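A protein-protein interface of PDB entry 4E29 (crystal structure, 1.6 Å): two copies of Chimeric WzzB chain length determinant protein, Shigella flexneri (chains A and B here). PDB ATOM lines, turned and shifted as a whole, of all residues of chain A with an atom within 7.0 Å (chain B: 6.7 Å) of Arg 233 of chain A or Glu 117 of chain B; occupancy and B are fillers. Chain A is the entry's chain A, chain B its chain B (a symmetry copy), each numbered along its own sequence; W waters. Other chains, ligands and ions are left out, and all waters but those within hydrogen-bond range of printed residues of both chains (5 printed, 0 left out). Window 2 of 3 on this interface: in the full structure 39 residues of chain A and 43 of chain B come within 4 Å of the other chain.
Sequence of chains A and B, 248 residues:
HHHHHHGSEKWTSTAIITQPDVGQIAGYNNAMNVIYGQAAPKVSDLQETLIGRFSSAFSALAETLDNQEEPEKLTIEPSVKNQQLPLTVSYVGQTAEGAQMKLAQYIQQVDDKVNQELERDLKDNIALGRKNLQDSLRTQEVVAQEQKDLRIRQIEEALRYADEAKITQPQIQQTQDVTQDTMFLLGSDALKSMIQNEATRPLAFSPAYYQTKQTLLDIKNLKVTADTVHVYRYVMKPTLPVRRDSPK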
ATOM      1  N   ILE A  16     -12.631 -10.397 -33.093  1.00  0.00           N
ATOM      2  CA  ILE A  16     -12.683 -11.823 -32.836  1.00  0.00           C
ATOM      3  C   ILE A  16     -12.538 -12.014 -31.337  1.00  0.00           C
ATOM      4  O   ILE A  16     -11.652 -11.436 -30.712  1.00  0.00           O
ATOM      5  CB  ILE A  16     -11.573 -12.587 -33.596  1.00  0.00           C
ATOM      6  CG1 ILE A  16     -11.777 -12.425 -35.113  1.00  0.00           C
ATOM      7  CG2 ILE A  16     -11.585 -14.054 -33.212  1.00  0.00           C
ATOM      8  CD1 ILE A  16     -10.591 -12.893 -35.945  1.00  0.00           C
ATOM      9  N   ILE A  17     -13.439 -12.798 -30.761  1.00  0.00           N
ATOM     10  CA  ILE A  17     -13.453 -13.021 -29.322  1.00  0.00           C
ATOM     11  C   ILE A  17     -13.509 -14.510 -29.038  1.00  0.00           C
ATOM     12  O   ILE A  17     -13.887 -15.305 -29.900  1.00  0.00           O
ATOM     13  CB  ILE A  17     -14.675 -12.354 -28.661  1.00  0.00           C
ATOM     14  CG1 ILE A  17     -15.967 -12.954 -29.215  1.00  0.00           C
ATOM     15  CG2 ILE A  17     -14.647 -10.848 -28.874  1.00  0.00           C
ATOM     16  CD1 ILE A  17     -17.230 -12.401 -28.561  1.00  0.00           C
ATOM     17  N   THR A  18     -13.133 -14.897 -27.828  1.00  0.00           N
ATOM     18  CA  THR A  18     -13.254 -16.282 -27.455  1.00  0.00           C
ATOM     19  C   THR A  18     -13.456 -16.390 -25.946  1.00  0.00           C
ATOM     20  O   THR A  18     -13.633 -15.381 -25.261  1.00  0.00           O
ATOM     21  CB  THR A  18     -12.036 -17.104 -27.922  1.00  0.00           C
ATOM     22  OG1 THR A  18     -12.332 -18.500 -27.783  1.00  0.00           O
ATOM     23  CG2 THR A  18     -10.792 -16.736 -27.107  1.00  0.00           C
ATOM     24  N   GLN A  19     -13.433 -17.613 -25.438  1.00  0.00           N
ATOM     25  CA  GLN A  19     -13.680 -17.851 -24.028  1.00  0.00           C
ATOM     26  C   GLN A  19     -12.645 -17.136 -23.156  1.00  0.00           C
ATOM     27  O   GLN A  19     -11.497 -16.961 -23.556  1.00  0.00           O
ATOM     28  CB  GLN A  19     -13.643 -19.355 -23.748  1.00  0.00           C
ATOM     29  CG  GLN A  19     -12.286 -19.986 -24.041  1.00  0.00           C
ATOM     30  CD  GLN A  19     -12.299 -21.497 -23.938  1.00  0.00           C
ATOM     31  OE1 GLN A  19     -13.358 -22.121 -23.906  1.00  0.00           O
ATOM     32  NE2 GLN A  19     -11.110 -22.096 -23.884  1.00  0.00           N
ATOM     33  N   PRO A  20     -13.055 -16.721 -21.952  1.00  0.00           N
ATOM     34  CA  PRO A  20     -12.129 -16.055 -21.033  1.00  0.00           C
ATOM     35  C   PRO A  20     -11.066 -17.036 -20.550  1.00  0.00           C
ATOM     36  O   PRO A  20     -11.313 -18.240 -20.525  1.00  0.00           O
ATOM     37  CB  PRO A  20     -13.032 -15.644 -19.873  1.00  0.00           C
ATOM     38  CG  PRO A  20     -14.125 -16.674 -19.878  1.00  0.00           C
ATOM     39  CD  PRO A  20     -14.376 -16.952 -21.338  1.00  0.00           C
ATOM     40  N   ASP A  21      -9.896 -16.529 -20.182  1.00  0.00           N
ATOM     41  CA  ASP A  21      -8.832 -17.399 -19.703  1.00  0.00           C
ATOM     42  C   ASP A  21      -9.074 -17.883 -18.284  1.00  0.00           C
ATOM     43  O   ASP A  21      -9.820 -17.266 -17.527  1.00  0.00           O
ATOM     44  CB  ASP A  21      -7.474 -16.711 -19.811  1.00  0.00           C
ATOM     45  CG  ASP A  21      -6.947 -16.716 -21.230  1.00  0.00           C
ATOM     46  OD1 ASP A  21      -7.129 -17.750 -21.909  1.00  0.00           O
ATOM     47  OD2 ASP A  21      -6.365 -15.702 -21.660  1.00  0.00           O
ATOM     48  N   ILE A  51     -18.646 -17.798 -22.216  1.00  0.00           N
ATOM     49  CA  ILE A  51     -18.639 -17.237 -23.569  1.00  0.00           C
ATOM     50  C   ILE A  51     -19.994 -17.474 -24.237  1.00  0.00           C
ATOM     51  O   ILE A  51     -20.487 -16.623 -24.977  1.00  0.00           O
ATOM     52  CB  ILE A  51     -17.479 -17.805 -24.434  1.00  0.00           C
ATOM     53  CG1 ILE A  51     -17.405 -17.092 -25.789  1.00  0.00           C
ATOM     54  CG2 ILE A  51     -17.648 -19.304 -24.635  1.00  0.00           C
ATOM     55  CD1 ILE A  51     -17.214 -15.585 -25.696  1.00  0.00           C
ATOM     56  N   HIS A 230     -15.102 -13.196 -15.872  1.00  0.00           N
ATOM     57  CA  HIS A 230     -15.087 -12.534 -17.168  1.00  0.00           C
ATOM     58  C   HIS A 230     -15.743 -13.507 -18.118  1.00  0.00           C
ATOM     59  O   HIS A 230     -15.834 -14.696 -17.807  1.00  0.00           O
ATOM     60  CB  HIS A 230     -13.660 -12.217 -17.598  1.00  0.00           C
ATOM     61  CG  HIS A 230     -13.002 -11.167 -16.762  1.00  0.00           C
ATOM     62  ND1 HIS A 230     -12.383 -11.450 -15.562  1.00  0.00           N
ATOM     63  CD2 HIS A 230     -12.876  -9.831 -16.943  1.00  0.00           C
ATOM     64  CE1 HIS A 230     -11.902 -10.336 -15.044  1.00  0.00           C
ATOM     65  NE2 HIS A 230     -12.186  -9.338 -15.862  1.00  0.00           N
ATOM     66  N   VAL A 231     -16.213 -13.022 -19.267  1.00  0.00           N
ATOM     67  CA  VAL A 231     -17.002 -13.875 -20.141  1.00  0.00           C
ATOM     68  C   VAL A 231     -16.449 -13.980 -21.552  1.00  0.00           C
ATOM     69  O   VAL A 231     -16.958 -14.756 -22.357  1.00  0.00           O
ATOM     70  CB  VAL A 231     -18.477 -13.423 -20.193  1.00  0.00           C
ATOM     71  CG1 VAL A 231     -19.118 -13.597 -18.829  1.00  0.00           C
ATOM     72  CG2 VAL A 231     -18.570 -11.976 -20.650  1.00  0.00           C
ATOM     73  N   TYR A 232     -15.410 -13.201 -21.847  1.00  0.00           N
ATOM     74  CA  TYR A 232     -14.778 -13.245 -23.159  1.00  0.00           C
ATOM     75  C   TYR A 232     -13.382 -12.652 -23.078  1.00  0.00           C
ATOM     76  O   TYR A 232     -13.046 -11.955 -22.125  1.00  0.00           O
ATOM     77  CB  TYR A 232     -15.599 -12.472 -24.204  1.00  0.00           C
ATOM     78  CG  TYR A 232     -15.293 -10.989 -24.232  1.00  0.00           C
ATOM     79  CD1 TYR A 232     -14.342 -10.473 -25.107  1.00  0.00           C
ATOM     80  CD2 TYR A 232     -15.938 -10.107 -23.370  1.00  0.00           C
ATOM     81  CE1 TYR A 232     -14.046  -9.122 -25.129  1.00  0.00           C
ATOM     82  CE2 TYR A 232     -15.651  -8.754 -23.387  1.00  0.00           C
ATOM     83  CZ  TYR A 232     -14.702  -8.270 -24.266  1.00  0.00           C
ATOM     84  OH  TYR A 232     -14.409  -6.929 -24.286  1.00  0.00           O
ATOM     85  N   ARG A 233     -12.565 -12.947 -24.080  1.00  0.00           N
ATOM     86  CA  ARG A 233     -11.331 -12.205 -24.285  1.00  0.00           C
ATOM     87  C   ARG A 233     -11.202 -11.886 -25.765  1.00  0.00           C
ATOM     88  O   ARG A 233     -11.746 -12.591 -26.614  1.00  0.00           O
ATOM     89  CB  ARG A 233     -10.115 -12.994 -23.795  1.00  0.00           C
ATOM     90  CG  ARG A 233      -9.740 -14.177 -24.671  1.00  0.00           C
ATOM     91  CD  ARG A 233      -8.449 -14.824 -24.191  1.00  0.00           C
ATOM     92  NE  ARG A 233      -8.073 -15.955 -25.032  1.00  0.00           N
ATOM     93  CZ  ARG A 233      -7.353 -15.853 -26.144  1.00  0.00           C
ATOM     94  NH1 ARG A 233      -6.931 -14.664 -26.561  1.00  0.00           N
ATOM     95  NH2 ARG A 233      -7.058 -16.941 -26.847  1.00  0.00           N
ATOM     96  N   TYR A 234     -10.484 -10.815 -26.074  1.00  0.00           N
ATOM     97  CA  TYR A 234     -10.228 -10.458 -27.458  1.00  0.00           C
ATOM     98  C   TYR A 234      -9.111 -11.302 -28.055  1.00  0.00           C
ATOM     99  O   TYR A 234      -8.010 -11.369 -27.508  1.00  0.00           O
ATOM    100  CB  TYR A 234      -9.834  -8.987 -27.564  1.00  0.00           C
ATOM    101  CG  TYR A 234     -10.986  -8.008 -27.617  1.00  0.00           C
ATOM    102  CD1 TYR A 234     -11.930  -8.066 -28.636  1.00  0.00           C
ATOM    103  CD2 TYR A 234     -11.110  -6.998 -26.668  1.00  0.00           C
ATOM    104  CE1 TYR A 234     -12.972  -7.158 -28.701  1.00  0.00           C
ATOM    105  CE2 TYR A 234     -12.149  -6.087 -26.724  1.00  0.00           C
ATOM    106  CZ  TYR A 234     -13.074  -6.169 -27.745  1.00  0.00           C
ATOM    107  OH  TYR A 234     -14.106  -5.260 -27.816  1.00  0.00           O
ATOM    108  N   VAL A 235      -9.404 -11.944 -29.178  1.00  0.00           N
ATOM    109  CA  VAL A 235      -8.351 -12.472 -30.035  1.00  0.00           C
ATOM    110  C   VAL A 235      -7.913 -11.351 -30.988  1.00  0.00           C
ATOM    111  O   VAL A 235      -6.737 -11.228 -31.320  1.00  0.00           O
ATOM    112  CB  VAL A 235      -8.820 -13.713 -30.829  1.00  0.00           C
ATOM    113  CG1 VAL A 235      -7.695 -14.266 -31.689  1.00  0.00           C
ATOM    114  CG2 VAL A 235      -9.339 -14.783 -29.879  1.00  0.00           C
ATOM    115  N   MET A 236      -8.872 -10.530 -31.411  1.00  0.00           N
ATOM    116  CA  MET A 236      -8.608  -9.343 -32.221  1.00  0.00           C
ATOM    117  C   MET A 236      -9.603  -8.247 -31.845  1.00  0.00           C
ATOM    118  O   MET A 236     -10.816  -8.465 -31.886  1.00  0.00           O
ATOM    119  CB  MET A 236      -8.747  -9.665 -33.709  1.00  0.00           C
ATOM    120  CG  MET A 236      -8.347  -8.513 -34.633  1.00  0.00           C
ATOM    121  SD  MET A 236      -8.653  -8.861 -36.529  1.00  0.00           S
ATOM    122  CE  MET A 236     -10.609  -8.885 -36.538  1.00  0.00           C
ATOM    123  N   ARG B  53      -4.439 -22.124 -29.430  1.00  0.00           N
ATOM    124  CA  ARG B  53      -4.377 -20.697 -29.116  1.00  0.00           C
ATOM    125  C   ARG B  53      -3.489 -19.941 -30.102  1.00  0.00           C
ATOM    126  O   ARG B  53      -3.812 -18.827 -30.521  1.00  0.00           O
ATOM    127  CB  ARG B  53      -3.878 -20.476 -27.685  1.00  0.00           C
ATOM    128  CG  ARG B  53      -3.987 -19.028 -27.218  1.00  0.00           C
ATOM    129  CD  ARG B  53      -3.369 -18.816 -25.848  1.00  0.00           C
ATOM    130  NE  ARG B  53      -3.668 -17.484 -25.329  1.00  0.00           N
ATOM    131  CZ  ARG B  53      -4.528 -17.254 -24.340  1.00  0.00           C
ATOM    132  NH1 ARG B  53      -5.147 -18.267 -23.752  1.00  0.00           N
ATOM    133  NH2 ARG B  53      -4.750 -16.018 -23.929  1.00  0.00           N
ATOM    134  N   SER B  56      -5.559 -19.697 -33.545  1.00  0.00           N
ATOM    135  CA  SER B  56      -6.610 -18.688 -33.652  1.00  0.00           C
ATOM    136  C   SER B  56      -6.003 -17.285 -33.691  1.00  0.00           C
ATOM    137  O   SER B  56      -6.505 -16.402 -34.390  1.00  0.00           O
ATOM    138  CB  SER B  56      -7.651 -18.824 -32.531  1.00  0.00           C
ATOM    139  OG  SER B  56      -7.091 -18.587 -31.255  1.00  0.00           O
ATOM    140  N   ALA B  57      -4.911 -17.090 -32.955  1.00  0.00           N
ATOM    141  CA  ALA B  57      -4.206 -15.811 -32.976  1.00  0.00           C
ATOM    142  C   ALA B  57      -3.592 -15.538 -34.345  1.00  0.00           C
ATOM    143  O   ALA B  57      -3.533 -14.392 -34.796  1.00  0.00           O
ATOM    144  CB  ALA B  57      -3.117 -15.780 -31.898  1.00  0.00           C
ATOM    145  N   ASP B 112       5.057 -14.252 -29.673  1.00  0.00           N
ATOM    146  CA  ASP B 112       5.343 -13.310 -28.594  1.00  0.00           C
ATOM    147  C   ASP B 112       4.056 -12.841 -27.922  1.00  0.00           C
ATOM    148  O   ASP B 112       3.979 -12.739 -26.697  1.00  0.00           O
ATOM    149  CB  ASP B 112       6.089 -12.091 -29.131  1.00  0.00           C
ATOM    150  CG  ASP B 112       7.535 -12.391 -29.502  1.00  0.00           C
ATOM    151  OD1 ASP B 112       8.079 -13.440 -29.091  1.00  0.00           O
ATOM    152  OD2 ASP B 112       8.132 -11.547 -30.199  1.00  0.00           O
ATOM    153  N   LYS B 113       3.052 -12.524 -28.730  1.00  0.00           N
ATOM    154  CA  LYS B 113       1.779 -12.049 -28.199  1.00  0.00           C
ATOM    155  C   LYS B 113       1.087 -13.085 -27.308  1.00  0.00           C
ATOM    156  O   LYS B 113       0.636 -12.765 -26.201  1.00  0.00           O
ATOM    157  CB  LYS B 113       0.840 -11.641 -29.333  1.00  0.00           C
ATOM    158  CG  LYS B 113      -0.521 -11.119 -28.853  1.00  0.00           C
ATOM    159  CD  LYS B 113      -1.391 -10.651 -30.023  1.00  0.00           C
ATOM    160  CE  LYS B 113      -2.582  -9.824 -29.538  1.00  0.00           C
ATOM    161  N   VAL B 114       0.997 -14.321 -27.794  1.00  0.00           N
ATOM    162  CA  VAL B 114       0.307 -15.385 -27.063  1.00  0.00           C
ATOM    163  C   VAL B 114       1.078 -15.753 -25.792  1.00  0.00           C
ATOM    164  O   VAL B 114       0.483 -15.986 -24.739  1.00  0.00           O
ATOM    165  CB  VAL B 114       0.069 -16.625 -27.952  1.00  0.00           C
ATOM    166  CG1 VAL B 114      -0.412 -17.801 -27.128  1.00  0.00           C
ATOM    167  CG2 VAL B 114      -0.938 -16.291 -29.058  1.00  0.00           C
ATOM    168  N   ASN B 115       2.403 -15.770 -25.885  1.00  0.00           N
ATOM    169  CA  ASN B 115       3.223 -16.099 -24.723  1.00  0.00           C
ATOM    170  C   ASN B 115       3.045 -15.070 -23.618  1.00  0.00           C
ATOM    171  O   ASN B 115       2.926 -15.421 -22.449  1.00  0.00           O
ATOM    172  CB  ASN B 115       4.699 -16.226 -25.105  1.00  0.00           C
ATOM    173  CG  ASN B 115       5.091 -17.656 -25.425  1.00  0.00           C
ATOM    174  OD1 ASN B 115       5.508 -18.403 -24.544  1.00  0.00           O
ATOM    175  ND2 ASN B 115       4.958 -18.044 -26.687  1.00  0.00           N
ATOM    176  N   GLN B 116       3.019 -13.795 -23.986  1.00  0.00           N
ATOM    177  CA  GLN B 116       2.831 -12.756 -22.985  1.00  0.00           C
ATOM    178  C   GLN B 116       1.475 -12.901 -22.295  1.00  0.00           C
ATOM    179  O   GLN B 116       1.384 -12.786 -21.075  1.00  0.00           O
ATOM    180  CB  GLN B 116       2.961 -11.367 -23.609  1.00  0.00           C
ATOM    181  CG  GLN B 116       2.784 -10.239 -22.604  1.00  0.00           C
ATOM    182  CD  GLN B 116       3.256  -8.903 -23.150  1.00  0.00           C
ATOM    183  OE1 GLN B 116       4.439  -8.727 -23.445  1.00  0.00           O
ATOM    184  NE2 GLN B 116       2.336  -7.955 -23.283  1.00  0.00           N
ATOM    185  N   GLU B 117       0.432 -13.170 -23.073  1.00  0.00           N
ATOM    186  CA  GLU B 117      -0.907 -13.355 -22.501  1.00  0.00           C
ATOM    187  C   GLU B 117      -0.943 -14.542 -21.546  1.00  0.00           C
ATOM    188  O   GLU B 117      -1.474 -14.448 -20.439  1.00  0.00           O
ATOM    189  CB  GLU B 117      -1.935 -13.565 -23.606  1.00  0.00           C
ATOM    190  CG  GLU B 117      -2.158 -12.347 -24.471  1.00  0.00           C
ATOM    191  CD  GLU B 117      -3.136 -12.612 -25.594  1.00  0.00           C
ATOM    192  OE1 GLU B 117      -3.331 -13.797 -25.957  1.00  0.00           O
ATOM    193  OE2 GLU B 117      -3.704 -11.631 -26.118  1.00  0.00           O
ATOM    194  N   LEU B 118      -0.386 -15.666 -21.972  1.00  0.00           N
ATOM    195  CA  LEU B 118      -0.366 -16.850 -21.117  1.00  0.00           C
ATOM    196  C   LEU B 118       0.431 -16.618 -19.828  1.00  0.00           C
ATOM    197  O   LEU B 118       0.038 -17.049 -18.747  1.00  0.00           O
ATOM    198  CB  LEU B 118       0.208 -18.044 -21.891  1.00  0.00           C
ATOM    199  CG  LEU B 118      -0.697 -18.639 -22.964  1.00  0.00           C
ATOM    200  CD1 LEU B 118       0.085 -19.582 -23.875  1.00  0.00           C
ATOM    201  CD2 LEU B 118      -1.902 -19.349 -22.338  1.00  0.00           C
ATOM    202  N   GLU B 119       1.563 -15.942 -19.947  1.00  0.00           N
ATOM    203  CA  GLU B 119       2.402 -15.665 -18.795  1.00  0.00           C
ATOM    204  C   GLU B 119       1.701 -14.760 -17.795  1.00  0.00           C
ATOM    205  O   GLU B 119       1.748 -15.004 -16.593  1.00  0.00           O
ATOM    206  CB  GLU B 119       3.722 -15.035 -19.238  1.00  0.00           C
ATOM    207  CG  GLU B 119       4.639 -16.019 -19.940  1.00  0.00           C
ATOM    208  CD  GLU B 119       5.795 -15.336 -20.637  1.00  0.00           C
ATOM    209  OE1 GLU B 119       6.242 -14.275 -20.153  1.00  0.00           O
ATOM    210  OE2 GLU B 119       6.249 -15.859 -21.673  1.00  0.00           O
ATOM    211  N   ARG B 120       1.049 -13.716 -18.289  1.00  0.00           N
ATOM    212  CA  ARG B 120       0.349 -12.795 -17.404  1.00  0.00           C
ATOM    213  C   ARG B 120      -0.840 -13.476 -16.750  1.00  0.00           C
ATOM    214  O   ARG B 120      -1.088 -13.288 -15.559  1.00  0.00           O
ATOM    215  CB  ARG B 120      -0.058 -11.529 -18.149  1.00  0.00           C
ATOM    216  CG  ARG B 120       1.152 -10.698 -18.525  1.00  0.00           C
ATOM    217  CD  ARG B 120       0.769  -9.436 -19.258  1.00  0.00           C
ATOM    218  NE  ARG B 120       1.944  -8.643 -19.604  1.00  0.00           N
ATOM    219  CZ  ARG B 120       1.893  -7.393 -20.051  1.00  0.00           C
ATOM    220  NH1 ARG B 120       0.720  -6.790 -20.200  1.00  0.00           N
ATOM    221  NH2 ARG B 120       3.013  -6.744 -20.342  1.00  0.00           N
ATOM    222  N   ASP B 121      -1.557 -14.292 -17.513  1.00  0.00           N
ATOM    223  CA  ASP B 121      -2.717 -14.977 -16.949  1.00  0.00           C
ATOM    224  C   ASP B 121      -2.285 -15.970 -15.875  1.00  0.00           C
ATOM    225  O   ASP B 121      -2.950 -16.114 -14.852  1.00  0.00           O
ATOM    226  CB  ASP B 121      -3.523 -15.697 -18.024  1.00  0.00           C
ATOM    227  CG  ASP B 121      -4.814 -16.281 -17.481  1.00  0.00           C
ATOM    228  OD1 ASP B 121      -5.690 -15.487 -17.089  1.00  0.00           O
ATOM    229  OD2 ASP B 121      -4.955 -17.522 -17.453  1.00  0.00           O
ATOM    230  N   LEU B 122      -1.167 -16.648 -16.108  1.00  0.00           N
ATOM    231  CA  LEU B 122      -0.651 -17.611 -15.146  1.00  0.00           C
ATOM    232  C   LEU B 122      -0.195 -16.926 -13.866  1.00  0.00           C
ATOM    233  O   LEU B 122      -0.428 -17.433 -12.762  1.00  0.00           O
ATOM    234  CB  LEU B 122       0.506 -18.405 -15.767  1.00  0.00           C
ATOM    235  CG  LEU B 122       1.143 -19.451 -14.851  1.00  0.00           C
ATOM    236  CD1 LEU B 122       0.065 -20.361 -14.279  1.00  0.00           C
ATOM    237  CD2 LEU B 122       2.209 -20.248 -15.596  1.00  0.00           C
HETATM  238  O   HOH W   1      -9.760 -19.284 -29.859  1.00  0.00           O
HETATM  239  O   HOH W   2      -5.849 -17.085 -29.563  1.00  0.00           O
HETATM  240  O   HOH W   3      -4.945 -14.637 -28.751  1.00  0.00           O
HETATM  241  O   HOH W   4      -5.421 -10.679 -27.783  1.00  0.00           O
HETATM  242  O   HOH W   5      -6.707 -12.239 -25.408  1.00  0.00           O
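The backbone NH (N) of Val 235 of chain A is in hydrogen-bond range of the backbone carbonyl oxygen (O) of Ile 16 of chain A, at 2.8 Å. OG of Ser 56 of chain B is in hydrogen-bond range of O of Arg 53 of chain B (3.4 Å). The side-chain carboxylate (OD1) of Asp 21 of chain A lies within salt-bridge range of the guanidinium group (NE) of Arg 233 of chain A. O of Thr 18 of chain A is in hydrogen-bond range of N of Arg 233 of chain A. NH2 of Arg 53 of chain B is in salt-bridge range of OE1 of Glu 117 of chain B (3.3 Å).
Of chain B, only Arg 53 (3.4 Å) and Glu 117 (3.8 Å) come within 4 Å of Arg 233 of chain A. Of chain A, only Arg 233 (3.8 Å) comes within 4 Å of Glu 117 of chain B. Of the printed residues of chain A, Arg 53 of chain B touches Asp 21 and Arg 233. Of the printed residues of chain B, Val 235 of chain A touches Ser 56. Printed residues of chain A within 4 Å of Asp 121 of chain B: Asp 21 (3.5 Å). Of the printed residues of chain B, Asp 21 of chain A touches Arg 53 and Asp 121. The nearest residue of chain A that does not touch Glu 117 of chain B is Tyr 234 of chain A (4.5 Å). The nearest printed residue of chain A that does not touch Ser 56 of chain B is Arg 233 of chain A (4.7 Å).
Of the 14 printed residues of chain A, 3 touch a printed residue of chain B. Hydrophobic or aromatic side chains of chain A within 4 Å of the printed part of chain B: Val 235. Along chain A the printed residues that touch a printed residue of chain B span positions 21 to 235. Among the printed residues, Asp or Glu carboxylates within 4 Å of a Lys or Arg side-chain nitrogen of the other chain: Asp 21 of chain A with Arg 53 of chain B (2.8 Å) and Arg 233 of chain A with Glu 117 of chain B (3.8 Å).
The guanidinium group of Arg 233 of chain A lies within salt-bridge range of the side-chain carboxylate of Glu 117 of chain B (3.8 Å). NH1 of Arg 53 of chain B is in salt-bridge range of OD1 of Asp 21 of chain A (2.8 Å).
CB of Asp 21 of chain A touches OD1 of Asp 121 of chain B, 3.5 Å away. Arg 53 of chain B touches Arg 233 of chain A (NH2 to CZ, 3.4 Å). O of Ser 56 of chain B touches CG1 of Val 235 of chain A (3.6 Å).
Water W4 bridges the side-chain carboxylate (OE2) of Glu 117 of chain B and the backbone carbonyl oxygen (O) of Tyr 234 of chain A. Water W2 lies within hydrogen-bond range of OG of Ser 56 of chain B, O of Arg 53 of chain B and NH2 of Arg 233 of chain A. Water W5 lies within hydrogen-bond range of the backbone carbonyl oxygen of Tyr 234 of chain A, the guanidinium group of Arg 233 of chain A and the side-chain carboxylate of Glu 117 of chain B. Water W3 bridges NH1 of Arg 233 of chain A and OE1 of Glu 117 of chain B. Water W1 bridges OG of Ser 56 of chain B (3.1 Å) and OG1 of Thr 18 of chain A (3.4 Å).
No position is printed for both chains.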
